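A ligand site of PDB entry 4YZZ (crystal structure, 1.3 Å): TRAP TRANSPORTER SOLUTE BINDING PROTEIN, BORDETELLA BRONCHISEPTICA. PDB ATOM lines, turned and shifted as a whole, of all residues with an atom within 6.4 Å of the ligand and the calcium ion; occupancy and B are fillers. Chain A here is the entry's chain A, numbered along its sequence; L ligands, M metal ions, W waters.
Water W1 lies within hydrogen-bond range of the backbone carbonyl oxygen (O) of Gly 180 (2.8 Å) and the side-chain carboxylate (OE1) of Glu 241 (2.8 Å). Water W2 bridges O2 of the ligand and OE1 of Gln 196.
The calcium ion is bound by the side-chain amide oxygen (OE1) of Gln 157 (2.3 Å), the backbone carbonyl oxygen (O) of Trp 216 (2.4 Å), an oxygen (O1) of the ligand (2.4 Å), water W1 (2.4 Å), the side-chain carboxylate (OE1) of Glu 215 (2.4 Å), the side-chain carboxylate (OE2) of Glu 215 (2.5 Å) and a nitrogen (N1) of the ligand (2.6 Å).
Of the 24 residues printed, 3 come within 4 Å of the calcium ion.
Trp 41 touches the ligand (CZ3 to C6, 3.8 Å). CD1 of Leu 98 touches C5 of the ligand, at 3.8 Å. Gly 180 touches the ligand (CA to O1, 3.5 Å). Ile 217 touches the ligand. Ala 244 touches the ligand. Ile 246 touches the ligand (CD1 to C3, 3.9 Å). Ten residues have an atom within 4 Å of the ligand: Trp 41, Leu 98, Gln 157, Arg 178, Gly 180, Glu 215, Trp 216, Ile 217, Ala 244 and Ile 246. The nearest printed residue that does not touch the ligand is Ile 48 (4.1 Å).
The guanidinium group of Arg 178 is in salt-bridge range of an oxygen (O2) of the ligand (2.9 Å).
The backbone NH of Met 158 is in hydrogen-bond range of the backbone carbonyl oxygen of Ile 217 (3.0 Å). OE2 of Glu 215 sits close to N of Gly 180 (3.0 Å). O of Ala 244 lies within hydrogen-bond range of N of Val 154, at 3.1 Å. The guanidinium group (NH1) of Arg 178 is in hydrogen-bond range of the backbone carbonyl oxygen (O) of Glu 215. NE2 of Gln 157 is in hydrogen-bond range of OE1 of Glu 241 (2.7 Å). NE of Arg 178 sits at hydrogen-bond distance from O of Ile 197, at 2.8 Å.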
ATOM      1  N   TRP A  41     -24.396  22.130  26.267  1.00  0.00           N
ATOM      2  CA  TRP A  41     -23.521  22.629  25.186  1.00  0.00           C
ATOM      3  C   TRP A  41     -22.202  23.204  25.654  1.00  0.00           C
ATOM      4  O   TRP A  41     -22.097  23.768  26.736  1.00  0.00           O
ATOM      5  CB  TRP A  41     -24.241  23.741  24.415  1.00  0.00           C
ATOM      6  CG  TRP A  41     -25.709  23.627  24.486  1.00  0.00           C
ATOM      7  CD1 TRP A  41     -26.566  24.520  25.047  1.00  0.00           C
ATOM      8  CD2 TRP A  41     -26.529  22.541  23.991  1.00  0.00           C
ATOM      9  NE1 TRP A  41     -27.851  24.062  24.949  1.00  0.00           N
ATOM     10  CE2 TRP A  41     -27.862  22.853  24.308  1.00  0.00           C
ATOM     11  CE3 TRP A  41     -26.260  21.340  23.339  1.00  0.00           C
ATOM     12  CZ2 TRP A  41     -28.916  21.999  23.994  1.00  0.00           C
ATOM     13  CZ3 TRP A  41     -27.310  20.498  23.022  1.00  0.00           C
ATOM     14  CH2 TRP A  41     -28.621  20.833  23.336  1.00  0.00           C
ATOM     15  N   ILE A  48     -26.171  28.222  20.028  1.00  0.00           N
ATOM     16  CA  ILE A  48     -27.055  27.532  20.977  1.00  0.00           C
ATOM     17  C   ILE A  48     -26.755  27.862  22.453  1.00  0.00           C
ATOM     18  O   ILE A  48     -27.686  28.169  23.220  1.00  0.00           O
ATOM     19  CB  ILE A  48     -27.109  26.006  20.689  1.00  0.00           C
ATOM     20  CG1 ILE A  48     -28.190  25.320  21.506  1.00  0.00           C
ATOM     21  CG2 ILE A  48     -25.757  25.337  20.877  1.00  0.00           C
ATOM     22  CD1 ILE A  48     -28.534  23.944  20.950  1.00  0.00           C
ATOM     23  N   VAL A  97     -31.689  21.765  26.589  1.00  0.00           N
ATOM     24  CA  VAL A  97     -31.363  20.433  26.099  1.00  0.00           C
ATOM     25  C   VAL A  97     -32.072  20.084  24.788  1.00  0.00           C
ATOM     26  O   VAL A  97     -33.014  20.733  24.332  1.00  0.00           O
ATOM     27  CB  VAL A  97     -31.757  19.337  27.143  1.00  0.00           C
ATOM     28  CG1 VAL A  97     -31.012  19.547  28.463  1.00  0.00           C
ATOM     29  CG2 VAL A  97     -33.273  19.288  27.378  1.00  0.00           C
ATOM     30  N   LEU A  98     -31.596  18.989  24.210  1.00  0.00           N
ATOM     31  CA  LEU A  98     -32.291  18.287  23.152  1.00  0.00           C
ATOM     32  C   LEU A  98     -33.056  17.181  23.844  1.00  0.00           C
ATOM     33  O   LEU A  98     -32.448  16.234  24.359  1.00  0.00           O
ATOM     34  CB  LEU A  98     -31.301  17.697  22.163  1.00  0.00           C
ATOM     35  CG  LEU A  98     -31.943  16.999  20.954  1.00  0.00           C
ATOM     36  CD1 LEU A  98     -32.097  18.023  19.854  1.00  0.00           C
ATOM     37  CD2 LEU A  98     -31.120  15.767  20.504  1.00  0.00           C
ATOM     38  N   MET A 101     -32.300  13.427  23.482  1.00  0.00           N
ATOM     39  CA  MET A 101     -31.184  12.754  24.144  1.00  0.00           C
ATOM     40  C   MET A 101     -31.716  11.754  25.170  1.00  0.00           C
ATOM     41  O   MET A 101     -31.086  10.725  25.444  1.00  0.00           O
ATOM     42  CB  MET A 101     -30.246  13.762  24.811  1.00  0.00           C
ATOM     43  CG  MET A 101     -29.043  13.041  25.392  1.00  0.00           C
ATOM     44  SD  MET A 101     -27.892  14.157  26.184  1.00  0.00           S
ATOM     45  CE  MET A 101     -26.477  13.072  26.362  1.00  0.00           C
ATOM     46  N   VAL A 154     -32.702  24.968  15.726  1.00  0.00           N
ATOM     47  CA  VAL A 154     -31.517  25.114  14.888  1.00  0.00           C
ATOM     48  C   VAL A 154     -31.835  24.934  13.405  1.00  0.00           C
ATOM     49  O   VAL A 154     -30.922  24.989  12.552  1.00  0.00           O
ATOM     50  CB  VAL A 154     -30.404  24.143  15.330  1.00  0.00           C
ATOM     51  CG1 VAL A 154     -30.194  24.210  16.825  1.00  0.00           C
ATOM     52  CG2 VAL A 154     -30.726  22.715  14.937  1.00  0.00           C
ATOM     53  N   GLN A 157     -30.837  20.520  10.026  1.00  0.00           N
ATOM     54  CA  GLN A 157     -29.436  20.227  10.262  1.00  0.00           C
ATOM     55  C   GLN A 157     -28.763  19.738   8.994  1.00  0.00           C
ATOM     56  O   GLN A 157     -29.417  19.422   8.000  1.00  0.00           O
ATOM     57  CB  GLN A 157     -29.350  19.165  11.340  1.00  0.00           C
ATOM     58  CG  GLN A 157     -29.887  19.649  12.673  1.00  0.00           C
ATOM     59  CD  GLN A 157     -30.179  18.510  13.580  1.00  0.00           C
ATOM     60  OE1 GLN A 157     -29.379  18.177  14.473  1.00  0.00           O
ATOM     61  NE2 GLN A 157     -31.325  17.866  13.366  1.00  0.00           N
ATOM     62  N   MET A 158     -27.427  19.719   9.011  1.00  0.00           N
ATOM     63  CA  MET A 158     -26.681  19.020   7.968  1.00  0.00           C
ATOM     64  C   MET A 158     -26.729  17.504   8.209  1.00  0.00           C
ATOM     65  O   MET A 158     -27.193  17.050   9.260  1.00  0.00           O
ATOM     66  CB  MET A 158     -25.252  19.550   7.894  1.00  0.00           C
ATOM     67  CG  MET A 158     -25.229  20.962   7.329  1.00  0.00           C
ATOM     68  SD  MET A 158     -25.663  21.035   5.565  1.00  0.00           S
ATOM     69  CE  MET A 158     -24.135  20.461   4.793  1.00  0.00           C
ATOM     70  N   ARG A 178     -21.906   8.910  15.299  1.00  0.00           N
ATOM     71  CA  ARG A 178     -22.495   9.760  16.331  1.00  0.00           C
ATOM     72  C   ARG A 178     -23.671  10.517  15.744  1.00  0.00           C
ATOM     73  O   ARG A 178     -23.552  11.203  14.736  1.00  0.00           O
ATOM     74  CB  ARG A 178     -21.459  10.759  16.839  1.00  0.00           C
ATOM     75  CG  ARG A 178     -21.916  11.609  18.031  1.00  0.00           C
ATOM     76  CD  ARG A 178     -22.659  12.868  17.650  1.00  0.00           C
ATOM     77  NE  ARG A 178     -23.327  13.366  18.841  1.00  0.00           N
ATOM     78  CZ  ARG A 178     -24.393  14.142  18.850  1.00  0.00           C
ATOM     79  NH1 ARG A 178     -24.931  14.615  17.743  1.00  0.00           N
ATOM     80  NH2 ARG A 178     -24.929  14.466  20.014  1.00  0.00           N
ATOM     81  N   ILE A 179     -24.809  10.408  16.410  1.00  0.00           N
ATOM     82  CA  ILE A 179     -26.011  11.133  15.989  1.00  0.00           C
ATOM     83  C   ILE A 179     -26.888  11.307  17.213  1.00  0.00           C
ATOM     84  O   ILE A 179     -27.097  10.374  17.982  1.00  0.00           O
ATOM     85  CB  ILE A 179     -26.759  10.380  14.848  1.00  0.00           C
ATOM     86  CG1 ILE A 179     -28.116  11.039  14.564  1.00  0.00           C
ATOM     87  CG2 ILE A 179     -26.922   8.907  15.147  1.00  0.00           C
ATOM     88  CD1 ILE A 179     -28.816  10.527  13.299  1.00  0.00           C
ATOM     89  N   GLY A 180     -27.386  12.526  17.390  1.00  0.00           N
ATOM     90  CA  GLY A 180     -28.334  12.814  18.456  1.00  0.00           C
ATOM     91  C   GLY A 180     -29.768  12.668  17.979  1.00  0.00           C
ATOM     92  O   GLY A 180     -30.057  12.820  16.795  1.00  0.00           O
ATOM     93  N   GLY A 181     -30.673  12.369  18.898  1.00  0.00           N
ATOM     94  CA  GLY A 181     -32.087  12.342  18.611  1.00  0.00           C
ATOM     95  C   GLY A 181     -32.626  11.045  18.019  1.00  0.00           C
ATOM     96  O   GLY A 181     -31.945  10.002  17.966  1.00  0.00           O
ATOM     97  N   GLN A 196     -25.334   8.711  20.931  1.00  0.00           N
ATOM     98  CA  GLN A 196     -25.549  10.126  21.266  1.00  0.00           C
ATOM     99  C   GLN A 196     -24.399  10.724  22.113  1.00  0.00           C
ATOM    100  O   GLN A 196     -24.615  11.258  23.185  1.00  0.00           O
ATOM    101  CB  GLN A 196     -26.904  10.327  21.993  1.00  0.00           C
ATOM    102  CG  GLN A 196     -28.105   9.820  21.207  1.00  0.00           C
ATOM    103  CD  GLN A 196     -29.370  10.617  21.471  1.00  0.00           C
ATOM    104  OE1 GLN A 196     -29.360  11.859  21.427  1.00  0.00           O
ATOM    105  NE2 GLN A 196     -30.449   9.928  21.747  1.00  0.00           N
ATOM    106  N   ILE A 197     -23.190  10.664  21.586  1.00  0.00           N
ATOM    107  CA  ILE A 197     -22.002  11.150  22.302  1.00  0.00           C
ATOM    108  C   ILE A 197     -22.145  12.677  22.472  1.00  0.00           C
ATOM    109  O   ILE A 197     -22.512  13.376  21.528  1.00  0.00           O
ATOM    110  CB  ILE A 197     -20.724  10.781  21.497  1.00  0.00           C
ATOM    111  CG1 ILE A 197     -20.503   9.253  21.450  1.00  0.00           C
ATOM    112  CG2 ILE A 197     -19.479  11.474  22.075  1.00  0.00           C
ATOM    113  CD1 ILE A 197     -19.599   8.795  20.335  1.00  0.00           C
ATOM    114  N   PRO A 199     -21.529  16.770  22.729  1.00  0.00           N
ATOM    115  CA  PRO A 199     -20.818  17.567  21.714  1.00  0.00           C
ATOM    116  C   PRO A 199     -19.320  17.686  21.927  1.00  0.00           C
ATOM    117  O   PRO A 199     -18.575  17.556  20.963  1.00  0.00           O
ATOM    118  CB  PRO A 199     -21.481  18.945  21.799  1.00  0.00           C
ATOM    119  CG  PRO A 199     -22.373  18.899  22.978  1.00  0.00           C
ATOM    120  CD  PRO A 199     -22.730  17.470  23.212  1.00  0.00           C
ATOM    121  N   GLU A 215     -22.728  13.465  13.045  1.00  0.00           N
ATOM    122  CA  GLU A 215     -23.506  14.678  12.785  1.00  0.00           C
ATOM    123  C   GLU A 215     -23.617  15.433  14.105  1.00  0.00           C
ATOM    124  O   GLU A 215     -23.636  14.837  15.182  1.00  0.00           O
ATOM    125  CB  GLU A 215     -24.888  14.330  12.210  1.00  0.00           C
ATOM    126  CG  GLU A 215     -25.885  13.739  13.199  1.00  0.00           C
ATOM    127  CD  GLU A 215     -26.654  14.778  14.029  1.00  0.00           C
ATOM    128  OE1 GLU A 215     -27.010  15.874  13.511  1.00  0.00           O
ATOM    129  OE2 GLU A 215     -26.930  14.494  15.195  1.00  0.00           O
ATOM    130  N   TRP A 216     -23.654  16.767  13.999  1.00  0.00           N
ATOM    131  CA  TRP A 216     -23.910  17.623  15.158  1.00  0.00           C
ATOM    132  C   TRP A 216     -25.079  18.548  14.814  1.00  0.00           C
ATOM    133  O   TRP A 216     -26.208  18.214  15.190  1.00  0.00           O
ATOM    134  CB  TRP A 216     -22.639  18.356  15.615  1.00  0.00           C
ATOM    135  CG  TRP A 216     -22.939  19.419  16.613  1.00  0.00           C
ATOM    136  CD1 TRP A 216     -22.779  20.769  16.455  1.00  0.00           C
ATOM    137  CD2 TRP A 216     -23.537  19.230  17.911  1.00  0.00           C
ATOM    138  NE1 TRP A 216     -23.232  21.432  17.580  1.00  0.00           N
ATOM    139  CE2 TRP A 216     -23.702  20.513  18.479  1.00  0.00           C
ATOM    140  CE3 TRP A 216     -23.955  18.106  18.639  1.00  0.00           C
ATOM    141  CZ2 TRP A 216     -24.263  20.700  19.745  1.00  0.00           C
ATOM    142  CZ3 TRP A 216     -24.491  18.297  19.877  1.00  0.00           C
ATOM    143  CH2 TRP A 216     -24.640  19.576  20.430  1.00  0.00           C
ATOM    144  N   ILE A 217     -24.834  19.660  14.111  1.00  0.00           N
ATOM    145  CA  ILE A 217     -25.898  20.623  13.783  1.00  0.00           C
ATOM    146  C   ILE A 217     -25.806  21.227  12.376  1.00  0.00           C
ATOM    147  O   ILE A 217     -26.751  21.137  11.577  1.00  0.00           O
ATOM    148  CB  ILE A 217     -25.951  21.776  14.809  1.00  0.00           C
ATOM    149  CG1 ILE A 217     -26.382  21.253  16.185  1.00  0.00           C
ATOM    150  CG2 ILE A 217     -26.931  22.841  14.351  1.00  0.00           C
ATOM    151  CD1 ILE A 217     -26.473  22.318  17.280  1.00  0.00           C
ATOM    152  N   PHE A 240     -32.889  13.888   9.970  1.00  0.00           N
ATOM    153  CA  PHE A 240     -33.014  13.332  11.321  1.00  0.00           C
ATOM    154  C   PHE A 240     -34.157  13.905  12.125  1.00  0.00           C
ATOM    155  O   PHE A 240     -34.851  13.201  12.849  1.00  0.00           O
ATOM    156  CB  PHE A 240     -31.689  13.557  12.087  1.00  0.00           C
ATOM    157  CG  PHE A 240     -30.448  13.294  11.267  1.00  0.00           C
ATOM    158  CD1 PHE A 240     -30.356  12.161  10.483  1.00  0.00           C
ATOM    159  CD2 PHE A 240     -29.376  14.192  11.243  1.00  0.00           C
ATOM    160  CE1 PHE A 240     -29.212  11.913   9.708  1.00  0.00           C
ATOM    161  CE2 PHE A 240     -28.241  13.939  10.467  1.00  0.00           C
ATOM    162  CZ  PHE A 240     -28.173  12.801   9.711  1.00  0.00           C
ATOM    163  N   GLU A 241     -34.336  15.208  11.983  1.00  0.00           N
ATOM    164  CA  GLU A 241     -35.515  15.931  12.464  1.00  0.00           C
ATOM    165  C   GLU A 241     -35.930  16.900  11.371  1.00  0.00           C
ATOM    166  O   GLU A 241     -35.094  17.408  10.638  1.00  0.00           O
ATOM    167  CB  GLU A 241     -35.209  16.745  13.735  1.00  0.00           C
ATOM    168  CG  GLU A 241     -35.041  15.930  15.022  1.00  0.00           C
ATOM    169  CD  GLU A 241     -33.638  15.408  15.313  1.00  0.00           C
ATOM    170  OE1 GLU A 241     -32.618  15.889  14.742  1.00  0.00           O
ATOM    171  OE2 GLU A 241     -33.543  14.484  16.144  1.00  0.00           O
ATOM    172  N   ALA A 244     -34.612  20.703  14.578  1.00  0.00           N
ATOM    173  CA  ALA A 244     -34.265  20.315  15.946  1.00  0.00           C
ATOM    174  C   ALA A 244     -34.619  21.434  16.912  1.00  0.00           C
ATOM    175  O   ALA A 244     -33.943  22.461  16.989  1.00  0.00           O
ATOM    176  CB  ALA A 244     -32.793  19.914  16.052  1.00  0.00           C
ATOM    177  N   SER A 245     -35.707  21.212  17.628  1.00  0.00           N
ATOM    178  CA  SER A 245     -36.220  22.164  18.602  1.00  0.00           C
ATOM    179  C   SER A 245     -35.548  21.926  19.938  1.00  0.00           C
ATOM    180  O   SER A 245     -35.248  20.780  20.308  1.00  0.00           O
ATOM    181  CB  SER A 245     -37.740  21.994  18.703  1.00  0.00           C
ATOM    182  OG  SER A 245     -38.325  22.981  19.525  1.00  0.00           O
ATOM    183  N   ILE A 246     -35.267  23.021  20.646  1.00  0.00           N
ATOM    184  CA  ILE A 246     -34.568  23.006  21.920  1.00  0.00           C
ATOM    185  C   ILE A 246     -35.541  23.282  23.055  1.00  0.00           C
ATOM    186  O   ILE A 246     -36.437  24.119  22.912  1.00  0.00           O
ATOM    187  CB  ILE A 246     -33.438  24.039  21.909  1.00  0.00           C
ATOM    188  CG1 ILE A 246     -32.560  23.887  20.660  1.00  0.00           C
ATOM    189  CG2 ILE A 246     -32.616  23.975  23.181  1.00  0.00           C
ATOM    190  CD1 ILE A 246     -31.893  22.504  20.481  1.00  0.00           C
ATOM    191  N   TYR A 281     -28.420  31.374  13.970  1.00  0.00           N
ATOM    192  CA  TYR A 281     -27.980  30.314  13.060  1.00  0.00           C
ATOM    193  C   TYR A 281     -28.143  30.712  11.588  1.00  0.00           C
ATOM    194  O   TYR A 281     -27.218  30.565  10.766  1.00  0.00           O
ATOM    195  CB  TYR A 281     -28.757  29.030  13.326  1.00  0.00           C
ATOM    196  CG  TYR A 281     -28.175  28.171  14.435  1.00  0.00           C
ATOM    197  CD1 TYR A 281     -26.934  27.565  14.289  1.00  0.00           C
ATOM    198  CD2 TYR A 281     -28.854  27.984  15.632  1.00  0.00           C
ATOM    199  CE1 TYR A 281     -26.389  26.773  15.282  1.00  0.00           C
ATOM    200  CE2 TYR A 281     -28.317  27.201  16.640  1.00  0.00           C
ATOM    201  CZ  TYR A 281     -27.083  26.613  16.469  1.00  0.00           C
ATOM    202  OH  TYR A 281     -26.586  25.838  17.479  1.00  0.00           O
HETATM  203  C1  LIG L   1     -28.094  17.984  18.703  1.00  0.00           C
HETATM  204  C2  LIG L   1     -29.220  19.558  17.300  1.00  0.00           C
HETATM  205  C3  LIG L   1     -29.378  20.425  18.376  1.00  0.00           C
HETATM  206  C4  LIG L   1     -27.513  16.706  18.797  1.00  0.00           C
HETATM  207  C5  LIG L   1     -28.898  20.075  19.623  1.00  0.00           C
HETATM  208  C6  LIG L   1     -28.307  18.816  19.822  1.00  0.00           C
HETATM  209  O1  LIG L   1     -27.338  16.044  17.727  1.00  0.00           O
HETATM  210  O2  LIG L   1     -27.287  16.164  19.909  1.00  0.00           O
HETATM  211  N1  LIG L   1     -28.561  18.345  17.480  1.00  0.00           N
HETATM  212 CA    CA M   1     -28.016  16.746  15.560  1.00  0.00          CA
HETATM  213  O   HOH W   1     -29.980  15.342  15.574  1.00  0.00           O
HETATM  214  O   HOH W   2     -27.983  14.349  21.980  1.00  0.00           O
